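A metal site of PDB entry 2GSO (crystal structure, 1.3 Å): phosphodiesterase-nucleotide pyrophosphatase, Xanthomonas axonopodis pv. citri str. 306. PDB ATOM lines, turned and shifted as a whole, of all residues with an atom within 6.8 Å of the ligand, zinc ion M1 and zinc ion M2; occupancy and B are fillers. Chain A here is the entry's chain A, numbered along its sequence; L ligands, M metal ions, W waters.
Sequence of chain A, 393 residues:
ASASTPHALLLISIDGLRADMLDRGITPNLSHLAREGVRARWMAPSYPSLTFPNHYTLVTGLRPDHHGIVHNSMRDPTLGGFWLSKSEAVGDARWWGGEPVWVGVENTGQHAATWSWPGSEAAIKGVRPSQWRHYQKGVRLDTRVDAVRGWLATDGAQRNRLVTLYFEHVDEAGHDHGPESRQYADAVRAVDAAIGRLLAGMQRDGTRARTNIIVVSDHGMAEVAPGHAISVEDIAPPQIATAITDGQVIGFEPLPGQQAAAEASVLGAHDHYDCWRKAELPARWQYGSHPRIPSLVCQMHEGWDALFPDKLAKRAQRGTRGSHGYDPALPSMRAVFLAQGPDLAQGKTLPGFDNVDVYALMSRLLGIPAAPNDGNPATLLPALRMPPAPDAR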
ATOM      1  N   ILE A  14      18.337  17.660 -32.263  1.00  0.00           N
ATOM      2  CA  ILE A  14      17.634  18.685 -33.005  1.00  0.00           C
ATOM      3  C   ILE A  14      16.167  18.567 -32.554  1.00  0.00           C
ATOM      4  O   ILE A  14      15.411  17.700 -33.027  1.00  0.00           O
ATOM      5  CB  ILE A  14      17.786  18.519 -34.527  1.00  0.00           C
ATOM      6  CG1 ILE A  14      19.275  18.466 -34.901  1.00  0.00           C
ATOM      7  CG2 ILE A  14      17.069  19.667 -35.231  1.00  0.00           C
ATOM      8  CD1 ILE A  14      19.546  18.100 -36.334  1.00  0.00           C
ATOM      9  N   ASP A  15      15.772  19.408 -31.609  1.00  0.00           N
ATOM     10  CA  ASP A  15      14.449  19.327 -31.018  1.00  0.00           C
ATOM     11  C   ASP A  15      13.364  19.385 -32.098  1.00  0.00           C
ATOM     12  O   ASP A  15      13.396  20.262 -32.967  1.00  0.00           O
ATOM     13  CB  ASP A  15      14.297  20.459 -29.983  1.00  0.00           C
ATOM     14  CG  ASP A  15      13.191  20.212 -29.000  1.00  0.00           C
ATOM     15  OD1 ASP A  15      12.164  19.682 -29.432  1.00  0.00           O
ATOM     16  OD2 ASP A  15      13.388  20.469 -27.793  1.00  0.00           O
ATOM     17  N   GLY A  16      12.430  18.438 -32.104  1.00  0.00           N
ATOM     18  CA  GLY A  16      11.268  18.500 -32.980  1.00  0.00           C
ATOM     19  C   GLY A  16      11.476  18.218 -34.449  1.00  0.00           C
ATOM     20  O   GLY A  16      10.613  18.534 -35.252  1.00  0.00           O
ATOM     21  N   SER A  49       5.116  12.152 -25.819  1.00  0.00           N
ATOM     22  CA  SER A  49       6.047  12.623 -26.868  1.00  0.00           C
ATOM     23  C   SER A  49       6.410  14.096 -26.696  1.00  0.00           C
ATOM     24  O   SER A  49       6.184  14.925 -27.601  1.00  0.00           O
ATOM     25  CB  SER A  49       5.484  12.357 -28.273  1.00  0.00           C
ATOM     26  OG  SER A  49       4.184  12.888 -28.402  1.00  0.00           O
ATOM     27  N   LEU A  50       6.972  14.402 -25.538  1.00  0.00           N
ATOM     28  CA  LEU A  50       7.311  15.746 -25.120  1.00  0.00           C
ATOM     29  C   LEU A  50       8.827  15.849 -24.885  1.00  0.00           C
ATOM     30  O   LEU A  50       9.526  14.834 -24.760  1.00  0.00           O
ATOM     31  CB  LEU A  50       6.541  16.122 -23.841  1.00  0.00           C
ATOM     32  CG  LEU A  50       5.015  16.159 -23.966  1.00  0.00           C
ATOM     33  CD1 LEU A  50       4.393  16.383 -22.612  1.00  0.00           C
ATOM     34  CD2 LEU A  50       4.592  17.232 -24.942  1.00  0.00           C
ATOM     35  N   THR A  51       9.332  17.077 -24.799  1.00  0.00           N
ATOM     36  CA  THR A  51      10.774  17.331 -24.789  1.00  0.00           C
ATOM     37  C   THR A  51      11.540  16.802 -23.609  1.00  0.00           C
ATOM     38  O   THR A  51      12.545  16.125 -23.794  1.00  0.00           O
ATOM     39  CB  THR A  51      11.012  18.833 -24.856  1.00  0.00           C
ATOM     40  OG1 THR A  51      10.484  19.305 -26.077  1.00  0.00           O
ATOM     41  CG2 THR A  51      12.497  19.194 -24.825  1.00  0.00           C
ATOM     42  N   PHE A  52      11.137  17.143 -22.399  1.00  0.00           N
ATOM     43  CA  PHE A  52      11.930  16.755 -21.246  1.00  0.00           C
ATOM     44  C   PHE A  52      11.889  15.241 -21.040  1.00  0.00           C
ATOM     45  O   PHE A  52      12.945  14.607 -20.900  1.00  0.00           O
ATOM     46  CB  PHE A  52      11.570  17.565 -19.985  1.00  0.00           C
ATOM     47  CG  PHE A  52      12.501  18.725 -19.735  1.00  0.00           C
ATOM     48  CD1 PHE A  52      12.871  19.589 -20.760  1.00  0.00           C
ATOM     49  CD2 PHE A  52      13.016  18.951 -18.465  1.00  0.00           C
ATOM     50  CE1 PHE A  52      13.737  20.661 -20.536  1.00  0.00           C
ATOM     51  CE2 PHE A  52      13.896  20.026 -18.230  1.00  0.00           C
ATOM     52  CZ  PHE A  52      14.250  20.865 -19.268  1.00  0.00           C
ATOM     53  N   PRO A  53      10.685  14.640 -21.062  1.00  0.00           N
ATOM     54  CA  PRO A  53      10.624  13.199 -20.950  1.00  0.00           C
ATOM     55  C   PRO A  53      11.510  12.454 -21.953  1.00  0.00           C
ATOM     56  O   PRO A  53      12.210  11.527 -21.594  1.00  0.00           O
ATOM     57  CB  PRO A  53       9.136  12.903 -21.148  1.00  0.00           C
ATOM     58  CG  PRO A  53       8.456  14.123 -20.629  1.00  0.00           C
ATOM     59  CD  PRO A  53       9.343  15.245 -21.077  1.00  0.00           C
ATOM     60  N   HIS A  55      14.112  13.638 -24.019  1.00  0.00           N
ATOM     61  CA  HIS A  55      15.542  13.880 -23.925  1.00  0.00           C
ATOM     62  C   HIS A  55      16.119  13.055 -22.770  1.00  0.00           C
ATOM     63  O   HIS A  55      17.227  12.527 -22.889  1.00  0.00           O
ATOM     64  CB  HIS A  55      15.888  15.354 -23.709  1.00  0.00           C
ATOM     65  CG  HIS A  55      15.940  16.161 -24.969  1.00  0.00           C
ATOM     66  ND1 HIS A  55      14.832  16.766 -25.499  1.00  0.00           N
ATOM     67  CD2 HIS A  55      16.967  16.455 -25.819  1.00  0.00           C
ATOM     68  CE1 HIS A  55      15.163  17.406 -26.612  1.00  0.00           C
ATOM     69  NE2 HIS A  55      16.449  17.227 -26.829  1.00  0.00           N
ATOM     70  N   ASN A  72       6.613  17.607 -19.070  1.00  0.00           N
ATOM     71  CA  ASN A  72       7.380  18.843 -18.903  1.00  0.00           C
ATOM     72  C   ASN A  72       6.971  19.610 -17.628  1.00  0.00           C
ATOM     73  O   ASN A  72       7.785  20.326 -17.064  1.00  0.00           O
ATOM     74  CB  ASN A  72       7.154  19.783 -20.094  1.00  0.00           C
ATOM     75  CG  ASN A  72       7.787  19.296 -21.391  1.00  0.00           C
ATOM     76  OD1 ASN A  72       8.787  18.576 -21.403  1.00  0.00           O
ATOM     77  ND2 ASN A  72       7.219  19.730 -22.511  1.00  0.00           N
ATOM     78  N   LEU A  84       9.571  23.882 -16.956  1.00  0.00           N
ATOM     79  CA  LEU A  84      10.845  24.100 -17.638  1.00  0.00           C
ATOM     80  C   LEU A  84      11.547  25.384 -17.205  1.00  0.00           C
ATOM     81  O   LEU A  84      12.774  25.442 -17.218  1.00  0.00           O
ATOM     82  CB  LEU A  84      10.671  24.036 -19.161  1.00  0.00           C
ATOM     83  CG  LEU A  84      10.030  22.756 -19.724  1.00  0.00           C
ATOM     84  CD1 LEU A  84      10.263  22.619 -21.228  1.00  0.00           C
ATOM     85  CD2 LEU A  84      10.539  21.502 -18.998  1.00  0.00           C
ATOM     86  N   TYR A 166      22.608  20.802 -28.402  1.00  0.00           N
ATOM     87  CA  TYR A 166      21.147  20.856 -28.462  1.00  0.00           C
ATOM     88  C   TYR A 166      20.736  22.055 -29.295  1.00  0.00           C
ATOM     89  O   TYR A 166      21.326  23.136 -29.135  1.00  0.00           O
ATOM     90  CB  TYR A 166      20.547  20.967 -27.067  1.00  0.00           C
ATOM     91  CG  TYR A 166      19.081  21.321 -27.049  1.00  0.00           C
ATOM     92  CD1 TYR A 166      18.102  20.359 -27.213  1.00  0.00           C
ATOM     93  CD2 TYR A 166      18.669  22.647 -26.896  1.00  0.00           C
ATOM     94  CE1 TYR A 166      16.760  20.686 -27.202  1.00  0.00           C
ATOM     95  CE2 TYR A 166      17.336  22.988 -26.892  1.00  0.00           C
ATOM     96  CZ  TYR A 166      16.386  22.012 -27.063  1.00  0.00           C
ATOM     97  OH  TYR A 166      15.046  22.348 -27.047  1.00  0.00           O
ATOM     98  N   ASP A 171      12.015  23.010 -33.477  1.00  0.00           N
ATOM     99  CA  ASP A 171      10.828  22.872 -32.644  1.00  0.00           C
ATOM    100  C   ASP A 171      10.065  24.190 -32.556  1.00  0.00           C
ATOM    101  O   ASP A 171       8.848  24.228 -32.707  1.00  0.00           O
ATOM    102  CB  ASP A 171      11.205  22.367 -31.246  1.00  0.00           C
ATOM    103  CG  ASP A 171      10.000  22.172 -30.371  1.00  0.00           C
ATOM    104  OD1 ASP A 171       9.247  21.210 -30.646  1.00  0.00           O
ATOM    105  OD2 ASP A 171       9.849  22.931 -29.387  1.00  0.00           O
ATOM    106  N   GLU A 172      10.777  25.286 -32.290  1.00  0.00           N
ATOM    107  CA  GLU A 172      10.144  26.590 -32.130  1.00  0.00           C
ATOM    108  C   GLU A 172       9.410  27.029 -33.393  1.00  0.00           C
ATOM    109  O   GLU A 172       8.277  27.490 -33.311  1.00  0.00           O
ATOM    110  CB  GLU A 172      11.170  27.637 -31.688  1.00  0.00           C
ATOM    111  CG  GLU A 172      11.742  27.363 -30.298  1.00  0.00           C
ATOM    112  CD  GLU A 172      12.549  28.527 -29.705  1.00  0.00           C
ATOM    113  OE1 GLU A 172      12.709  29.576 -30.376  1.00  0.00           O
ATOM    114  OE2 GLU A 172      13.030  28.385 -28.559  1.00  0.00           O
ATOM    115  N   HIS A 175       6.193  24.849 -33.780  1.00  0.00           N
ATOM    116  CA  HIS A 175       5.071  25.317 -32.973  1.00  0.00           C
ATOM    117  C   HIS A 175       4.418  26.558 -33.561  1.00  0.00           C
ATOM    118  O   HIS A 175       3.192  26.665 -33.624  1.00  0.00           O
ATOM    119  CB  HIS A 175       5.486  25.612 -31.538  1.00  0.00           C
ATOM    120  CG  HIS A 175       5.792  24.395 -30.732  1.00  0.00           C
ATOM    121  ND1 HIS A 175       4.824  23.507 -30.326  1.00  0.00           N
ATOM    122  CD2 HIS A 175       6.972  23.921 -30.252  1.00  0.00           C
ATOM    123  CE1 HIS A 175       5.399  22.534 -29.620  1.00  0.00           C
ATOM    124  NE2 HIS A 175       6.698  22.770 -29.562  1.00  0.00           N
ATOM    125  N   ASP A 218      13.999  14.394 -30.329  1.00  0.00           N
ATOM    126  CA  ASP A 218      13.185  13.906 -29.217  1.00  0.00           C
ATOM    127  C   ASP A 218      11.799  13.440 -29.651  1.00  0.00           C
ATOM    128  O   ASP A 218      11.225  12.566 -29.027  1.00  0.00           O
ATOM    129  CB  ASP A 218      13.121  14.958 -28.102  1.00  0.00           C
ATOM    130  CG  ASP A 218      12.686  16.323 -28.565  1.00  0.00           C
ATOM    131  OD1 ASP A 218      12.665  16.644 -29.778  1.00  0.00           O
ATOM    132  OD2 ASP A 218      12.314  17.073 -27.639  1.00  0.00           O
ATOM    133  N   HIS A 219      11.305  14.031 -30.727  1.00  0.00           N
ATOM    134  CA  HIS A 219       9.979  13.738 -31.277  1.00  0.00           C
ATOM    135  C   HIS A 219       9.825  14.512 -32.579  1.00  0.00           C
ATOM    136  O   HIS A 219      10.655  15.378 -32.893  1.00  0.00           O
ATOM    137  CB  HIS A 219       8.896  14.244 -30.332  1.00  0.00           C
ATOM    138  CG  HIS A 219       9.118  15.655 -29.918  1.00  0.00           C
ATOM    139  ND1 HIS A 219       8.913  16.718 -30.785  1.00  0.00           N
ATOM    140  CD2 HIS A 219       9.636  16.178 -28.788  1.00  0.00           C
ATOM    141  CE1 HIS A 219       9.282  17.832 -30.169  1.00  0.00           C
ATOM    142  NE2 HIS A 219       9.715  17.534 -28.963  1.00  0.00           N
ATOM    143  N   GLY A 220       8.771  14.210 -33.324  1.00  0.00           N
ATOM    144  CA  GLY A 220       8.433  14.944 -34.543  1.00  0.00           C
ATOM    145  C   GLY A 220       7.518  16.130 -34.270  1.00  0.00           C
ATOM    146  O   GLY A 220       7.649  16.805 -33.260  1.00  0.00           O
ATOM    147  N   MET A 221       6.642  16.420 -35.224  1.00  0.00           N
ATOM    148  CA  MET A 221       5.804  17.608 -35.187  1.00  0.00           C
ATOM    149  C   MET A 221       4.619  17.415 -36.103  1.00  0.00           C
ATOM    150  O   MET A 221       4.791  16.979 -37.239  1.00  0.00           O
ATOM    151  CB  MET A 221       6.617  18.805 -35.672  1.00  0.00           C
ATOM    152  CG  MET A 221       5.914  20.145 -35.565  1.00  0.00           C
ATOM    153  SD  MET A 221       5.728  20.744 -33.878  1.00  0.00           S
ATOM    154  CE  MET A 221       7.454  20.978 -33.450  1.00  0.00           C
ATOM    155  N   GLN A 248      -1.411  18.710 -25.004  1.00  0.00           N
ATOM    156  CA  GLN A 248      -1.871  17.475 -25.658  1.00  0.00           C
ATOM    157  C   GLN A 248      -2.010  16.287 -24.701  1.00  0.00           C
ATOM    158  O   GLN A 248      -2.835  15.408 -24.947  1.00  0.00           O
ATOM    159  CB  GLN A 248      -0.901  17.133 -26.793  1.00  0.00           C
ATOM    160  CG  GLN A 248      -0.749  18.281 -27.769  1.00  0.00           C
ATOM    161  CD  GLN A 248       0.205  19.361 -27.293  1.00  0.00           C
ATOM    162  OE1 GLN A 248       1.189  19.083 -26.604  1.00  0.00           O
ATOM    163  NE2 GLN A 248      -0.088  20.612 -27.642  1.00  0.00           N
ATOM    164  N   SER A 323       2.213  21.086 -33.172  1.00  0.00           N
ATOM    165  CA  SER A 323       2.303  20.485 -31.857  1.00  0.00           C
ATOM    166  C   SER A 323       2.823  19.072 -31.966  1.00  0.00           C
ATOM    167  O   SER A 323       2.770  18.432 -33.028  1.00  0.00           O
ATOM    168  CB  SER A 323       0.935  20.447 -31.160  1.00  0.00           C
ATOM    169  OG  SER A 323       0.465  21.714 -30.803  1.00  0.00           O
ATOM    170  N   HIS A 324       3.327  18.592 -30.843  1.00  0.00           N
ATOM    171  CA  HIS A 324       3.626  17.186 -30.675  1.00  0.00           C
ATOM    172  C   HIS A 324       2.956  16.754 -29.397  1.00  0.00           C
ATOM    173  O   HIS A 324       1.917  17.326 -29.059  1.00  0.00           O
ATOM    174  CB  HIS A 324       5.134  16.955 -30.736  1.00  0.00           C
ATOM    175  CG  HIS A 324       5.919  17.886 -29.881  1.00  0.00           C
ATOM    176  ND1 HIS A 324       6.338  17.535 -28.619  1.00  0.00           N
ATOM    177  CD2 HIS A 324       6.316  19.165 -30.075  1.00  0.00           C
ATOM    178  CE1 HIS A 324       6.974  18.557 -28.077  1.00  0.00           C
ATOM    179  NE2 HIS A 324       6.970  19.556 -28.940  1.00  0.00           N
ATOM    180  N   GLY A 325       3.446  15.742 -28.690  1.00  0.00           N
ATOM    181  CA  GLY A 325       2.714  15.248 -27.521  1.00  0.00           C
ATOM    182  C   GLY A 325       1.588  14.298 -27.866  1.00  0.00           C
ATOM    183  O   GLY A 325       0.761  13.969 -27.017  1.00  0.00           O
HETATM  184  V1  LIG L   1       9.172  20.666 -26.018  1.00  0.00           V
HETATM  185  O1  LIG L   1       7.772  19.484 -25.242  1.00  0.00           O
HETATM  186  O2  LIG L   1       9.853  21.799 -24.842  1.00  0.00           O
HETATM  187  O3  LIG L   1       9.752  20.573 -27.956  1.00  0.00           O
HETATM  188  O4  LIG L   1       7.754  21.811 -26.694  1.00  0.00           O
HETATM  189 ZN    ZN M   1       7.999  21.384 -28.834  1.00  0.00          ZN
HETATM  190 ZN    ZN M   2      11.058  18.724 -27.991  1.00  0.00          ZN
HETATM  191  O   HOH W   1      11.716  23.580 -24.255  1.00  0.00           O
HETATM  192  O   HOH W   2      11.482  22.464 -26.702  1.00  0.00           O
HETATM  193  O   HOH W   3       7.529  24.575 -25.898  1.00  0.00           O
HETATM  194  O   HOH W   4       5.160  20.622 -26.182  1.00  0.00           O
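A vanadium atom (V1) of the ligand is bound by the side-chain hydroxyl (OG1) of Thr 51, 1.9 Å away.
The side-chain carboxylate (OD2) of Asp 15 is in hydrogen-bond range of the side-chain hydroxyl (OH) of Tyr 166 (2.6 Å). OD2 of Asp 218 lies close to ND1 of His 55 (3.3 Å). O of His 324 sits close to OE1 of Gln 248, at 3.1 Å. ND1 of His 324 sits close to ND1 of His 219 (3.5 Å). The backbone carbonyl oxygen of Ser 49 is in hydrogen-bond range of a ring nitrogen (ND1) of His 324, 2.8 Å away. OD1 of Asn 72 lies within hydrogen-bond range of N of Phe 52 (2.9 Å). The backbone carbonyl oxygen of Asp 15 sits at hydrogen-bond distance from the backbone NH of Asp 171, 3.1 Å away. The backbone carbonyl oxygen of Thr 51 is in hydrogen-bond range of a ring nitrogen (ND1) of His 55, 2.9 Å away.
ND2 of Asn 72 lies close to O1 of the ligand. Residues that only touch the ligand: Leu 84 (3.7 Å) and Leu 50 (3.8 Å). Of the 23 residues printed, 9 come within 4 Å of the ligand. Along chain A the residues within 4 Å of the ligand span positions 15 to 324.
The nearest printed residue that does not touch zinc ion M1 is His 219 (4.01 Å).
Of the 23 residues printed, 4 come within 4 Å of zinc ion M2.
Zinc ion M1 is bound by a ring nitrogen (NE2) of His 175 (2.0 Å), a ring nitrogen (NE2) of His 324 (2.1 Å), an oxygen (O3) of the ligand (2.1 Å), an oxygen (O4) of the ligand (2.2 Å), the side-chain carboxylate (OD1) of Asp 171 (2.2 Å) and the side-chain carboxylate (OD2) of Asp 171 (2.5 Å).
Zinc ion M2 is bound by NE2 of His 219, OD1 of Asp 15, OG1 of Thr 51, OD2 of Asp 218 and O3 of the ligand. Zinc ion M2 has five donor atoms within binding distance.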
